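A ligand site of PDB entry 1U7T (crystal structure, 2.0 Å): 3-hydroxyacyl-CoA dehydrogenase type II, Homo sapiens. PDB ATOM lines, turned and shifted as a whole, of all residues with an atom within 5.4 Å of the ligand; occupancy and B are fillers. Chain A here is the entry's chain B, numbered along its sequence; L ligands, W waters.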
ATOM      1  N   GLY A  17     -25.474  31.577   8.719  1.00  0.00           N
ATOM      2  CA  GLY A  17     -26.590  30.750   8.259  1.00  0.00           C
ATOM      3  C   GLY A  17     -27.629  30.603   9.360  1.00  0.00           C
ATOM      4  O   GLY A  17     -28.432  29.659   9.415  1.00  0.00           O
ATOM      5  N   GLY A  18     -27.625  31.553  10.297  1.00  0.00           N
ATOM      6  CA  GLY A  18     -28.476  31.445  11.464  1.00  0.00           C
ATOM      7  C   GLY A  18     -29.958  31.597  11.159  1.00  0.00           C
ATOM      8  O   GLY A  18     -30.776  31.327  12.048  1.00  0.00           O
ATOM      9  N   ALA A  19     -30.338  32.006   9.955  1.00  0.00           N
ATOM     10  CA  ALA A  19     -31.755  32.162   9.639  1.00  0.00           C
ATOM     11  C   ALA A  19     -32.442  30.828   9.384  1.00  0.00           C
ATOM     12  O   ALA A  19     -33.669  30.697   9.379  1.00  0.00           O
ATOM     13  CB  ALA A  19     -31.926  33.078   8.440  1.00  0.00           C
ATOM     14  N   SER A  20     -31.656  29.773   9.151  1.00  0.00           N
ATOM     15  CA  SER A  20     -32.274  28.527   8.696  1.00  0.00           C
ATOM     16  C   SER A  20     -31.495  27.303   9.132  1.00  0.00           C
ATOM     17  O   SER A  20     -30.377  27.386   9.664  1.00  0.00           O
ATOM     18  CB  SER A  20     -32.371  28.598   7.168  1.00  0.00           C
ATOM     19  OG  SER A  20     -32.856  27.387   6.603  1.00  0.00           O
ATOM     20  N   GLY A  21     -32.098  26.144   8.917  1.00  0.00           N
ATOM     21  CA  GLY A  21     -31.517  24.844   9.028  1.00  0.00           C
ATOM     22  C   GLY A  21     -30.594  24.613  10.184  1.00  0.00           C
ATOM     23  O   GLY A  21     -30.999  24.728  11.343  1.00  0.00           O
ATOM     24  N   LEU A  22     -29.333  24.257   9.891  1.00  0.00           N
ATOM     25  CA  LEU A  22     -28.452  23.882  11.004  1.00  0.00           C
ATOM     26  C   LEU A  22     -28.127  25.084  11.892  1.00  0.00           C
ATOM     27  O   LEU A  22     -28.142  24.958  13.117  1.00  0.00           O
ATOM     28  CB  LEU A  22     -27.176  23.243  10.447  1.00  0.00           C
ATOM     29  CG  LEU A  22     -27.377  21.942   9.658  1.00  0.00           C
ATOM     30  CD1 LEU A  22     -26.045  21.412   9.140  1.00  0.00           C
ATOM     31  CD2 LEU A  22     -28.080  20.899  10.508  1.00  0.00           C
ATOM     32  N   GLY A  23     -27.841  26.232  11.296  1.00  0.00           N
ATOM     33  CA  GLY A  23     -27.494  27.399  12.109  1.00  0.00           C
ATOM     34  C   GLY A  23     -28.644  27.812  13.011  1.00  0.00           C
ATOM     35  O   GLY A  23     -28.485  28.057  14.208  1.00  0.00           O
ATOM     36  N   LEU A  40     -26.269  35.518  11.911  1.00  0.00           N
ATOM     37  CA  LEU A  40     -25.602  36.169  10.775  1.00  0.00           C
ATOM     38  C   LEU A  40     -26.097  35.538   9.482  1.00  0.00           C
ATOM     39  O   LEU A  40     -25.856  34.354   9.216  1.00  0.00           O
ATOM     40  CB  LEU A  40     -24.081  36.026  10.936  1.00  0.00           C
ATOM     41  CG  LEU A  40     -23.212  37.000  10.137  1.00  0.00           C
ATOM     42  CD1 LEU A  40     -21.838  37.126  10.782  1.00  0.00           C
ATOM     43  CD2 LEU A  40     -23.081  36.580   8.672  1.00  0.00           C
ATOM     44  N   ASP A  41     -26.798  36.305   8.657  1.00  0.00           N
ATOM     45  CA  ASP A  41     -27.391  35.719   7.448  1.00  0.00           C
ATOM     46  C   ASP A  41     -27.697  36.819   6.442  1.00  0.00           C
ATOM     47  O   ASP A  41     -27.482  38.007   6.706  1.00  0.00           O
ATOM     48  CB  ASP A  41     -28.629  34.908   7.812  1.00  0.00           C
ATOM     49  CG  ASP A  41     -28.870  33.739   6.874  1.00  0.00           C
ATOM     50  OD1 ASP A  41     -28.794  33.953   5.637  1.00  0.00           O
ATOM     51  OD2 ASP A  41     -29.132  32.606   7.345  1.00  0.00           O
ATOM     52  N   LEU A  42     -28.185  36.444   5.257  1.00  0.00           N
ATOM     53  CA  LEU A  42     -28.443  37.440   4.211  1.00  0.00           C
ATOM     54  C   LEU A  42     -29.675  38.259   4.569  1.00  0.00           C
ATOM     55  O   LEU A  42     -30.580  37.807   5.277  1.00  0.00           O
ATOM     56  CB  LEU A  42     -28.576  36.758   2.854  1.00  0.00           C
ATOM     57  CG  LEU A  42     -27.302  36.027   2.362  1.00  0.00           C
ATOM     58  CD1 LEU A  42     -27.587  35.160   1.145  1.00  0.00           C
ATOM     59  CD2 LEU A  42     -26.204  37.029   2.050  1.00  0.00           C
ATOM     60  N   SER A  45     -33.378  37.000   3.863  1.00  0.00           N
ATOM     61  CA  SER A  45     -33.822  35.808   4.555  1.00  0.00           C
ATOM     62  C   SER A  45     -34.808  36.174   5.663  1.00  0.00           C
ATOM     63  O   SER A  45     -35.122  37.347   5.857  1.00  0.00           O
ATOM     64  CB  SER A  45     -32.591  35.112   5.129  1.00  0.00           C
ATOM     65  OG  SER A  45     -31.948  35.920   6.112  1.00  0.00           O
ATOM     66  N   ALA A  63     -25.637  40.063   6.794  1.00  0.00           N
ATOM     67  CA  ALA A  63     -24.286  40.065   6.252  1.00  0.00           C
ATOM     68  C   ALA A  63     -24.109  38.954   5.216  1.00  0.00           C
ATOM     69  O   ALA A  63     -24.680  37.868   5.361  1.00  0.00           O
ATOM     70  CB  ALA A  63     -23.272  39.888   7.367  1.00  0.00           C
ATOM     71  N   ASP A  64     -23.318  39.244   4.195  1.00  0.00           N
ATOM     72  CA  ASP A  64     -22.812  38.236   3.264  1.00  0.00           C
ATOM     73  C   ASP A  64     -21.418  37.824   3.717  1.00  0.00           C
ATOM     74  O   ASP A  64     -20.553  38.693   3.832  1.00  0.00           O
ATOM     75  CB  ASP A  64     -22.792  38.787   1.856  1.00  0.00           C
ATOM     76  CG  ASP A  64     -22.328  37.791   0.810  1.00  0.00           C
ATOM     77  OD1 ASP A  64     -22.602  38.058  -0.374  1.00  0.00           O
ATOM     78  OD2 ASP A  64     -21.710  36.770   1.148  1.00  0.00           O
ATOM     79  N   VAL A  65     -21.192  36.527   3.989  1.00  0.00           N
ATOM     80  CA  VAL A  65     -19.913  36.109   4.557  1.00  0.00           C
ATOM     81  C   VAL A  65     -18.774  36.241   3.549  1.00  0.00           C
ATOM     82  O   VAL A  65     -17.608  36.171   3.930  1.00  0.00           O
ATOM     83  CB  VAL A  65     -19.919  34.672   5.101  1.00  0.00           C
ATOM     84  CG1 VAL A  65     -20.916  34.513   6.242  1.00  0.00           C
ATOM     85  CG2 VAL A  65     -20.205  33.670   3.991  1.00  0.00           C
ATOM     86  N   THR A  66     -19.100  36.426   2.269  1.00  0.00           N
ATOM     87  CA  THR A  66     -18.026  36.618   1.295  1.00  0.00           C
ATOM     88  C   THR A  66     -17.542  38.061   1.284  1.00  0.00           C
ATOM     89  O   THR A  66     -16.628  38.393   0.525  1.00  0.00           O
ATOM     90  CB  THR A  66     -18.468  36.252  -0.134  1.00  0.00           C
ATOM     91  OG1 THR A  66     -19.533  37.135  -0.521  1.00  0.00           O
ATOM     92  CG2 THR A  66     -18.991  34.828  -0.214  1.00  0.00           C
ATOM     93  N   ASN A  90     -19.845  28.512  11.882  1.00  0.00           N
ATOM     94  CA  ASN A  90     -19.988  28.728  10.454  1.00  0.00           C
ATOM     95  C   ASN A  90     -20.970  27.718   9.845  1.00  0.00           C
ATOM     96  O   ASN A  90     -20.648  26.545   9.624  1.00  0.00           O
ATOM     97  CB  ASN A  90     -18.622  28.604   9.768  1.00  0.00           C
ATOM     98  CG  ASN A  90     -17.716  29.773  10.132  1.00  0.00           C
ATOM     99  OD1 ASN A  90     -16.772  29.649  10.921  1.00  0.00           O
ATOM    100  ND2 ASN A  90     -17.998  30.932   9.558  1.00  0.00           N
ATOM    101  N   CYS A  91     -22.197  28.167   9.570  1.00  0.00           N
ATOM    102  CA  CYS A  91     -23.184  27.276   8.953  1.00  0.00           C
ATOM    103  C   CYS A  91     -23.572  27.770   7.572  1.00  0.00           C
ATOM    104  O   CYS A  91     -24.099  27.017   6.760  1.00  0.00           O
ATOM    105  CB  CYS A  91     -24.419  27.161   9.855  1.00  0.00           C
ATOM    106  SG  CYS A  91     -24.198  26.120  11.315  1.00  0.00           S
ATOM    107  N   ALA A  92     -23.304  29.045   7.281  1.00  0.00           N
ATOM    108  CA  ALA A  92     -23.545  29.603   5.955  1.00  0.00           C
ATOM    109  C   ALA A  92     -22.959  28.727   4.857  1.00  0.00           C
ATOM    110  O   ALA A  92     -21.770  28.381   4.867  1.00  0.00           O
ATOM    111  CB  ALA A  92     -22.958  31.016   5.877  1.00  0.00           C
ATOM    112  N   GLY A  93     -23.799  28.346   3.899  1.00  0.00           N
ATOM    113  CA  GLY A  93     -23.331  27.513   2.806  1.00  0.00           C
ATOM    114  C   GLY A  93     -24.321  27.394   1.663  1.00  0.00           C
ATOM    115  O   GLY A  93     -25.510  27.662   1.821  1.00  0.00           O
ATOM    116  N   ILE A  94     -23.845  26.986   0.490  1.00  0.00           N
ATOM    117  CA  ILE A  94     -24.692  26.711  -0.652  1.00  0.00           C
ATOM    118  C   ILE A  94     -24.318  25.357  -1.257  1.00  0.00           C
ATOM    119  O   ILE A  94     -23.260  24.813  -0.955  1.00  0.00           O
ATOM    120  CB  ILE A  94     -24.602  27.762  -1.771  1.00  0.00           C
ATOM    121  CG1 ILE A  94     -23.161  28.018  -2.234  1.00  0.00           C
ATOM    122  CG2 ILE A  94     -25.287  29.057  -1.383  1.00  0.00           C
ATOM    123  CD1 ILE A  94     -23.102  28.713  -3.586  1.00  0.00           C
ATOM    124  N   VAL A 120     -18.606  31.073  -1.325  1.00  0.00           N
ATOM    125  CA  VAL A 120     -19.451  31.099  -0.132  1.00  0.00           C
ATOM    126  C   VAL A 120     -18.969  30.115   0.931  1.00  0.00           C
ATOM    127  O   VAL A 120     -18.849  30.463   2.096  1.00  0.00           O
ATOM    128  CB  VAL A 120     -20.928  30.798  -0.441  1.00  0.00           C
ATOM    129  CG1 VAL A 120     -21.740  30.749   0.840  1.00  0.00           C
ATOM    130  CG2 VAL A 120     -21.503  31.835  -1.397  1.00  0.00           C
ATOM    131  N   ASN A 121     -18.741  28.866   0.536  1.00  0.00           N
ATOM    132  CA  ASN A 121     -18.530  27.803   1.503  1.00  0.00           C
ATOM    133  C   ASN A 121     -17.161  27.850   2.182  1.00  0.00           C
ATOM    134  O   ASN A 121     -17.101  27.593   3.389  1.00  0.00           O
ATOM    135  CB  ASN A 121     -18.665  26.427   0.825  1.00  0.00           C
ATOM    136  CG  ASN A 121     -20.104  26.051   0.547  1.00  0.00           C
ATOM    137  OD1 ASN A 121     -20.987  26.895   0.685  1.00  0.00           O
ATOM    138  ND2 ASN A 121     -20.348  24.804   0.171  1.00  0.00           N
ATOM    139  N   THR A 153     -18.629  24.049   9.537  1.00  0.00           N
ATOM    140  CA  THR A 153     -19.475  22.990   9.008  1.00  0.00           C
ATOM    141  C   THR A 153     -18.874  22.496   7.699  1.00  0.00           C
ATOM    142  O   THR A 153     -18.818  23.249   6.728  1.00  0.00           O
ATOM    143  CB  THR A 153     -20.931  23.441   8.773  1.00  0.00           C
ATOM    144  OG1 THR A 153     -21.450  23.981  10.002  1.00  0.00           O
ATOM    145  CG2 THR A 153     -21.802  22.245   8.404  1.00  0.00           C
ATOM    146  N   ALA A 154     -18.395  21.255   7.717  1.00  0.00           N
ATOM    147  CA  ALA A 154     -17.890  20.665   6.476  1.00  0.00           C
ATOM    148  C   ALA A 154     -19.042  19.850   5.875  1.00  0.00           C
ATOM    149  O   ALA A 154     -20.134  20.413   5.732  1.00  0.00           O
ATOM    150  CB  ALA A 154     -16.652  19.812   6.713  1.00  0.00           C
ATOM    151  N   SER A 155     -18.777  18.589   5.578  1.00  0.00           N
ATOM    152  CA  SER A 155     -19.768  17.656   5.062  1.00  0.00           C
ATOM    153  C   SER A 155     -19.117  16.303   4.811  1.00  0.00           C
ATOM    154  O   SER A 155     -17.923  16.234   4.555  1.00  0.00           O
ATOM    155  CB  SER A 155     -20.378  18.187   3.761  1.00  0.00           C
ATOM    156  OG  SER A 155     -21.044  17.151   3.061  1.00  0.00           O
ATOM    157  N   VAL A 156     -19.864  15.200   4.843  1.00  0.00           N
ATOM    158  CA  VAL A 156     -19.230  13.931   4.485  1.00  0.00           C
ATOM    159  C   VAL A 156     -18.771  13.940   3.027  1.00  0.00           C
ATOM    160  O   VAL A 156     -17.900  13.130   2.659  1.00  0.00           O
ATOM    161  CB  VAL A 156     -20.153  12.741   4.724  1.00  0.00           C
ATOM    162  CG1 VAL A 156     -20.466  12.592   6.213  1.00  0.00           C
ATOM    163  CG2 VAL A 156     -21.436  12.903   3.917  1.00  0.00           C
ATOM    164  N   TYR A 168     -18.810  21.369  -4.483  1.00  0.00           N
ATOM    165  CA  TYR A 168     -19.166  21.274  -3.079  1.00  0.00           C
ATOM    166  C   TYR A 168     -18.109  20.497  -2.305  1.00  0.00           C
ATOM    167  O   TYR A 168     -17.688  20.933  -1.232  1.00  0.00           O
ATOM    168  CB  TYR A 168     -20.525  20.590  -2.944  1.00  0.00           C
ATOM    169  CG  TYR A 168     -21.176  20.614  -1.582  1.00  0.00           C
ATOM    170  CD1 TYR A 168     -21.761  21.772  -1.080  1.00  0.00           C
ATOM    171  CD2 TYR A 168     -21.216  19.480  -0.787  1.00  0.00           C
ATOM    172  CE1 TYR A 168     -22.352  21.791   0.174  1.00  0.00           C
ATOM    173  CE2 TYR A 168     -21.805  19.492   0.461  1.00  0.00           C
ATOM    174  CZ  TYR A 168     -22.382  20.651   0.935  1.00  0.00           C
ATOM    175  OH  TYR A 168     -22.967  20.642   2.176  1.00  0.00           O
ATOM    176  N   LYS A 172     -15.831  21.732   0.821  1.00  0.00           N
ATOM    177  CA  LYS A 172     -15.904  21.142   2.163  1.00  0.00           C
ATOM    178  C   LYS A 172     -14.588  20.464   2.540  1.00  0.00           C
ATOM    179  O   LYS A 172     -14.221  20.422   3.716  1.00  0.00           O
ATOM    180  CB  LYS A 172     -17.103  20.184   2.265  1.00  0.00           C
ATOM    181  CG  LYS A 172     -18.445  20.904   2.130  1.00  0.00           C
ATOM    182  CD  LYS A 172     -18.604  22.037   3.135  1.00  0.00           C
ATOM    183  CE  LYS A 172     -20.006  22.604   3.137  1.00  0.00           C
ATOM    184  NZ  LYS A 172     -20.256  23.534   4.290  1.00  0.00           N
ATOM    185  N   PRO A 198     -21.519  17.042   8.609  1.00  0.00           N
ATOM    186  CA  PRO A 198     -22.844  16.410   8.571  1.00  0.00           C
ATOM    187  C   PRO A 198     -22.997  15.458   7.382  1.00  0.00           C
ATOM    188  O   PRO A 198     -22.460  15.698   6.314  1.00  0.00           O
ATOM    189  CB  PRO A 198     -23.789  17.597   8.411  1.00  0.00           C
ATOM    190  CG  PRO A 198     -23.003  18.781   8.867  1.00  0.00           C
ATOM    191  CD  PRO A 198     -21.589  18.489   8.382  1.00  0.00           C
ATOM    192  N   GLY A 199     -23.747  14.376   7.537  1.00  0.00           N
ATOM    193  CA  GLY A 199     -24.117  13.554   6.393  1.00  0.00           C
ATOM    194  C   GLY A 199     -25.394  14.106   5.747  1.00  0.00           C
ATOM    195  O   GLY A 199     -25.324  15.121   5.054  1.00  0.00           O
ATOM    196  N   LEU A 200     -26.530  13.463   5.972  1.00  0.00           N
ATOM    197  CA  LEU A 200     -27.803  13.903   5.413  1.00  0.00           C
ATOM    198  C   LEU A 200     -28.770  14.354   6.512  1.00  0.00           C
ATOM    199  O   LEU A 200     -29.129  13.564   7.379  1.00  0.00           O
ATOM    200  CB  LEU A 200     -28.483  12.788   4.628  1.00  0.00           C
ATOM    201  CG  LEU A 200     -27.735  12.083   3.509  1.00  0.00           C
ATOM    202  CD1 LEU A 200     -28.456  10.783   3.180  1.00  0.00           C
ATOM    203  CD2 LEU A 200     -27.609  12.988   2.288  1.00  0.00           C
ATOM    204  N   PHE A 201     -29.157  15.622   6.454  1.00  0.00           N
ATOM    205  CA  PHE A 201     -29.955  16.224   7.513  1.00  0.00           C
ATOM    206  C   PHE A 201     -31.237  16.861   6.983  1.00  0.00           C
ATOM    207  O   PHE A 201     -31.267  17.403   5.876  1.00  0.00           O
ATOM    208  CB  PHE A 201     -29.138  17.318   8.217  1.00  0.00           C
ATOM    209  CG  PHE A 201     -28.377  16.788   9.421  1.00  0.00           C
ATOM    210  CD1 PHE A 201     -27.217  16.051   9.234  1.00  0.00           C
ATOM    211  CD2 PHE A 201     -28.825  17.035  10.709  1.00  0.00           C
ATOM    212  CE1 PHE A 201     -26.522  15.567  10.325  1.00  0.00           C
ATOM    213  CE2 PHE A 201     -28.131  16.543  11.807  1.00  0.00           C
ATOM    214  CZ  PHE A 201     -26.979  15.813  11.611  1.00  0.00           C
ATOM    215  N   GLY A 202     -32.275  16.792   7.800  1.00  0.00           N
ATOM    216  CA  GLY A 202     -33.546  17.366   7.397  1.00  0.00           C
ATOM    217  C   GLY A 202     -33.583  18.858   7.575  1.00  0.00           C
ATOM    218  O   GLY A 202     -34.344  19.356   8.401  1.00  0.00           O
ATOM    219  N   THR A 203     -32.812  19.607   6.798  1.00  0.00           N
ATOM    220  CA  THR A 203     -32.976  21.057   6.728  1.00  0.00           C
ATOM    221  C   THR A 203     -33.770  21.366   5.462  1.00  0.00           C
ATOM    222  O   THR A 203     -33.963  20.384   4.730  1.00  0.00           O
ATOM    223  CB  THR A 203     -31.633  21.782   6.677  1.00  0.00           C
ATOM    224  OG1 THR A 203     -31.059  21.542   5.379  1.00  0.00           O
ATOM    225  CG2 THR A 203     -30.640  21.279   7.709  1.00  0.00           C
ATOM    226  N   PRO A 204     -34.226  22.573   5.178  1.00  0.00           N
ATOM    227  CA  PRO A 204     -34.984  22.834   3.943  1.00  0.00           C
ATOM    228  C   PRO A 204     -34.322  22.259   2.694  1.00  0.00           C
ATOM    229  O   PRO A 204     -35.019  21.886   1.745  1.00  0.00           O
ATOM    230  CB  PRO A 204     -35.013  24.362   3.853  1.00  0.00           C
ATOM    231  CG  PRO A 204     -35.011  24.782   5.288  1.00  0.00           C
ATOM    232  CD  PRO A 204     -34.144  23.789   6.001  1.00  0.00           C
ATOM    233  N   LEU A 205     -33.003  22.182   2.706  1.00  0.00           N
ATOM    234  CA  LEU A 205     -32.232  21.571   1.632  1.00  0.00           C
ATOM    235  C   LEU A 205     -32.773  20.203   1.269  1.00  0.00           C
ATOM    236  O   LEU A 205     -32.827  19.830   0.092  1.00  0.00           O
ATOM    237  CB  LEU A 205     -30.775  21.503   2.092  1.00  0.00           C
ATOM    238  CG  LEU A 205     -29.623  21.317   1.135  1.00  0.00           C
ATOM    239  CD1 LEU A 205     -29.832  21.983  -0.217  1.00  0.00           C
ATOM    240  CD2 LEU A 205     -28.357  21.876   1.786  1.00  0.00           C
ATOM    241  N   LEU A 206     -33.213  19.408   2.246  1.00  0.00           N
ATOM    242  CA  LEU A 206     -33.702  18.071   1.912  1.00  0.00           C
ATOM    243  C   LEU A 206     -35.196  17.912   2.172  1.00  0.00           C
ATOM    244  O   LEU A 206     -35.906  17.241   1.406  1.00  0.00           O
ATOM    245  CB  LEU A 206     -32.944  17.009   2.734  1.00  0.00           C
ATOM    246  CG  LEU A 206     -31.433  17.205   2.824  1.00  0.00           C
ATOM    247  CD1 LEU A 206     -30.780  16.003   3.491  1.00  0.00           C
ATOM    248  CD2 LEU A 206     -30.835  17.462   1.451  1.00  0.00           C
HETATM  249  P1  LIG L   1     -29.926  26.044   4.801  1.00  0.00           P
HETATM  250  O1  LIG L   1     -29.911  26.375   3.380  1.00  0.00           O
HETATM  251  O2  LIG L   1     -31.076  25.592   5.574  1.00  0.00           O
HETATM  252  O3  LIG L   1     -29.219  27.287   5.536  1.00  0.00           O
HETATM  253  C1  LIG L   1     -28.082  27.858   4.826  1.00  0.00           C
HETATM  254  C2  LIG L   1     -28.051  29.263   5.381  1.00  0.00           C
HETATM  255  O4  LIG L   1     -26.893  29.871   4.816  1.00  0.00           O
HETATM  256  C3  LIG L   1     -29.287  30.016   4.851  1.00  0.00           C
HETATM  257  O5  LIG L   1     -29.958  30.760   5.909  1.00  0.00           O
HETATM  258  C4  LIG L   1     -28.660  30.899   3.816  1.00  0.00           C
HETATM  259  O6  LIG L   1     -29.361  32.113   3.591  1.00  0.00           O
HETATM  260  C5  LIG L   1     -27.275  31.152   4.437  1.00  0.00           C
HETATM  261  N1  LIG L   1     -26.335  31.748   3.491  1.00  0.00           N
HETATM  262  C6  LIG L   1     -26.107  31.355   2.236  1.00  0.00           C
HETATM  263  N2  LIG L   1     -25.191  32.140   1.645  1.00  0.00           N
HETATM  264  C7  LIG L   1     -24.868  33.023   2.608  1.00  0.00           C
HETATM  265  C8  LIG L   1     -23.945  34.051   2.477  1.00  0.00           C
HETATM  266  N3  LIG L   1     -23.259  34.271   1.361  1.00  0.00           N
HETATM  267  N4  LIG L   1     -23.761  34.842   3.548  1.00  0.00           N
HETATM  268  C9  LIG L   1     -24.449  34.629   4.670  1.00  0.00           C
HETATM  269  N5  LIG L   1     -25.326  33.639   4.778  1.00  0.00           N
HETATM  270  C10 LIG L   1     -25.563  32.810   3.758  1.00  0.00           C
HETATM  271  O7  LIG L   1     -28.849  24.899   5.004  1.00  0.00           O
HETATM  272  P2  LIG L   1     -28.402  24.019   6.213  1.00  0.00           P
HETATM  273  O8  LIG L   1     -28.861  22.606   6.011  1.00  0.00           O
HETATM  274  O9  LIG L   1     -28.646  24.645   7.517  1.00  0.00           O
HETATM  275  O10 LIG L   1     -26.810  23.964   5.940  1.00  0.00           O
HETATM  276  C11 LIG L   1     -25.923  24.503   6.957  1.00  0.00           C
HETATM  277  C12 LIG L   1     -24.514  23.992   6.724  1.00  0.00           C
HETATM  278  O11 LIG L   1     -24.600  22.550   6.762  1.00  0.00           O
HETATM  279  C13 LIG L   1     -24.025  24.371   5.309  1.00  0.00           C
HETATM  280  O12 LIG L   1     -22.610  24.625   5.322  1.00  0.00           O
HETATM  281  C14 LIG L   1     -24.297  23.094   4.470  1.00  0.00           C
HETATM  282  O13 LIG L   1     -23.425  23.090   3.322  1.00  0.00           O
HETATM  283  C15 LIG L   1     -23.963  22.080   5.544  1.00  0.00           C
HETATM  284  N6  LIG L   1     -24.365  20.684   5.285  1.00  0.00           N
HETATM  285  C16 LIG L   1     -25.725  20.305   5.211  1.00  0.00           C
HETATM  286  C17 LIG L   1     -26.084  18.996   4.965  1.00  0.00           C
HETATM  287  C18 LIG L   1     -27.543  18.569   4.922  1.00  0.00           C
HETATM  288  O14 LIG L   1     -27.858  17.517   4.384  1.00  0.00           O
HETATM  289  N7  LIG L   1     -28.422  19.378   5.508  1.00  0.00           N
HETATM  290  C19 LIG L   1     -25.060  17.890   4.744  1.00  0.00           C
HETATM  291  C20 LIG L   1     -23.635  18.393   4.859  1.00  0.00           C
HETATM  292  C21 LIG L   1     -23.358  19.719   5.135  1.00  0.00           C
HETATM  293  O   HOH W   1     -27.643  26.875   8.413  1.00  0.00           O
HETATM  294  O   HOH W   2     -25.312  32.888  -0.730  1.00  0.00           O
HETATM  295  O   HOH W   3     -32.580  31.301   4.641  1.00  0.00           O
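The side-chain carboxylate of Asp 41 lies within hydrogen-bond range of an oxygen (O5) of the ligand. The backbone NH of Leu 22 is in hydrogen-bond range of an oxygen (O9) of the ligand. OG1 of Thr 203 sits at hydrogen-bond distance from O8 of the ligand (2.5 Å). The side-chain hydroxyl (OG) of Ser 20 lies within hydrogen-bond range of an oxygen (O2) of the ligand (2.7 Å). The side-chain hydroxyl of Tyr 168 sits at hydrogen-bond distance from an oxygen (O13) of the ligand, 2.7 Å away. NZ of Lys 172 is in hydrogen-bond range of O12 of the ligand (2.8 Å). The side-chain carboxylate (OD2) of Asp 64 lies within hydrogen-bond range of a nitrogen (N3) of the ligand, at 2.9 Å. The backbone carbonyl oxygen (O) of Cys 91 lies close to an oxygen (O12) of the ligand (3.2 Å). N of Phe 201 is in hydrogen-bond range of O14 of the ligand, 3.1 Å away. The backbone carbonyl oxygen (O) of Phe 201 lies close to a nitrogen (N7) of the ligand. N of Val 65 sits at hydrogen-bond distance from N4 of the ligand, at 3.1 Å.
N of Ala 63 sits at hydrogen-bond distance from O of Asp 41 (2.8 Å). N of Gly 18 sits at hydrogen-bond distance from OD2 of Asp 41, at 3.5 Å. The backbone carbonyl oxygen (O) of Thr 153 lies within hydrogen-bond range of the side-chain amino group (NZ) of Lys 172, at 2.8 Å. The backbone carbonyl oxygen of Ala 154 sits close to the side-chain amino group of Lys 172, 3.4 Å away. The side-chain hydroxyl of Thr 66 is in hydrogen-bond range of the side-chain carboxylate of Asp 64. The backbone NH of Gly 23 lies close to the side-chain sulfur of Cys 91 (3.6 Å). OG1 of Thr 153 sits at hydrogen-bond distance from O of Asn 90 (2.7 Å). The backbone NH (N) of Val 156 lies within hydrogen-bond range of the backbone carbonyl oxygen (O) of Pro 198 (3.0 Å).
Residues that only touch the ligand: Gly 199, Gly 21, Thr 153, Pro 198, Ala 63, Ala 154, Ser 155, Leu 206, Ala 92, Gly 17, Gly 93, Pro 204, Leu 42, Leu 200, Val 120 and Ala 19. Hydrophobic or aromatic side chains that line the ligand: Ala 19, Leu 22, Leu 42, Val 65, Ala 92, Val 120, Tyr 168, Pro 198, Phe 201, Pro 204 and Leu 206. The nearest printed residue that does not touch the ligand is Gly 23 (4.2 Å).
Water W1 lies within hydrogen-bond range of an oxygen (O9) of the ligand (2.6 Å), the backbone NH of Gly 23 (3.0 Å), the backbone carbonyl oxygen of Ser 20 (3.0 Å), the backbone carbonyl oxygen of Gly 17 (3.1 Å) and the backbone NH of Leu 22 (3.4 Å).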
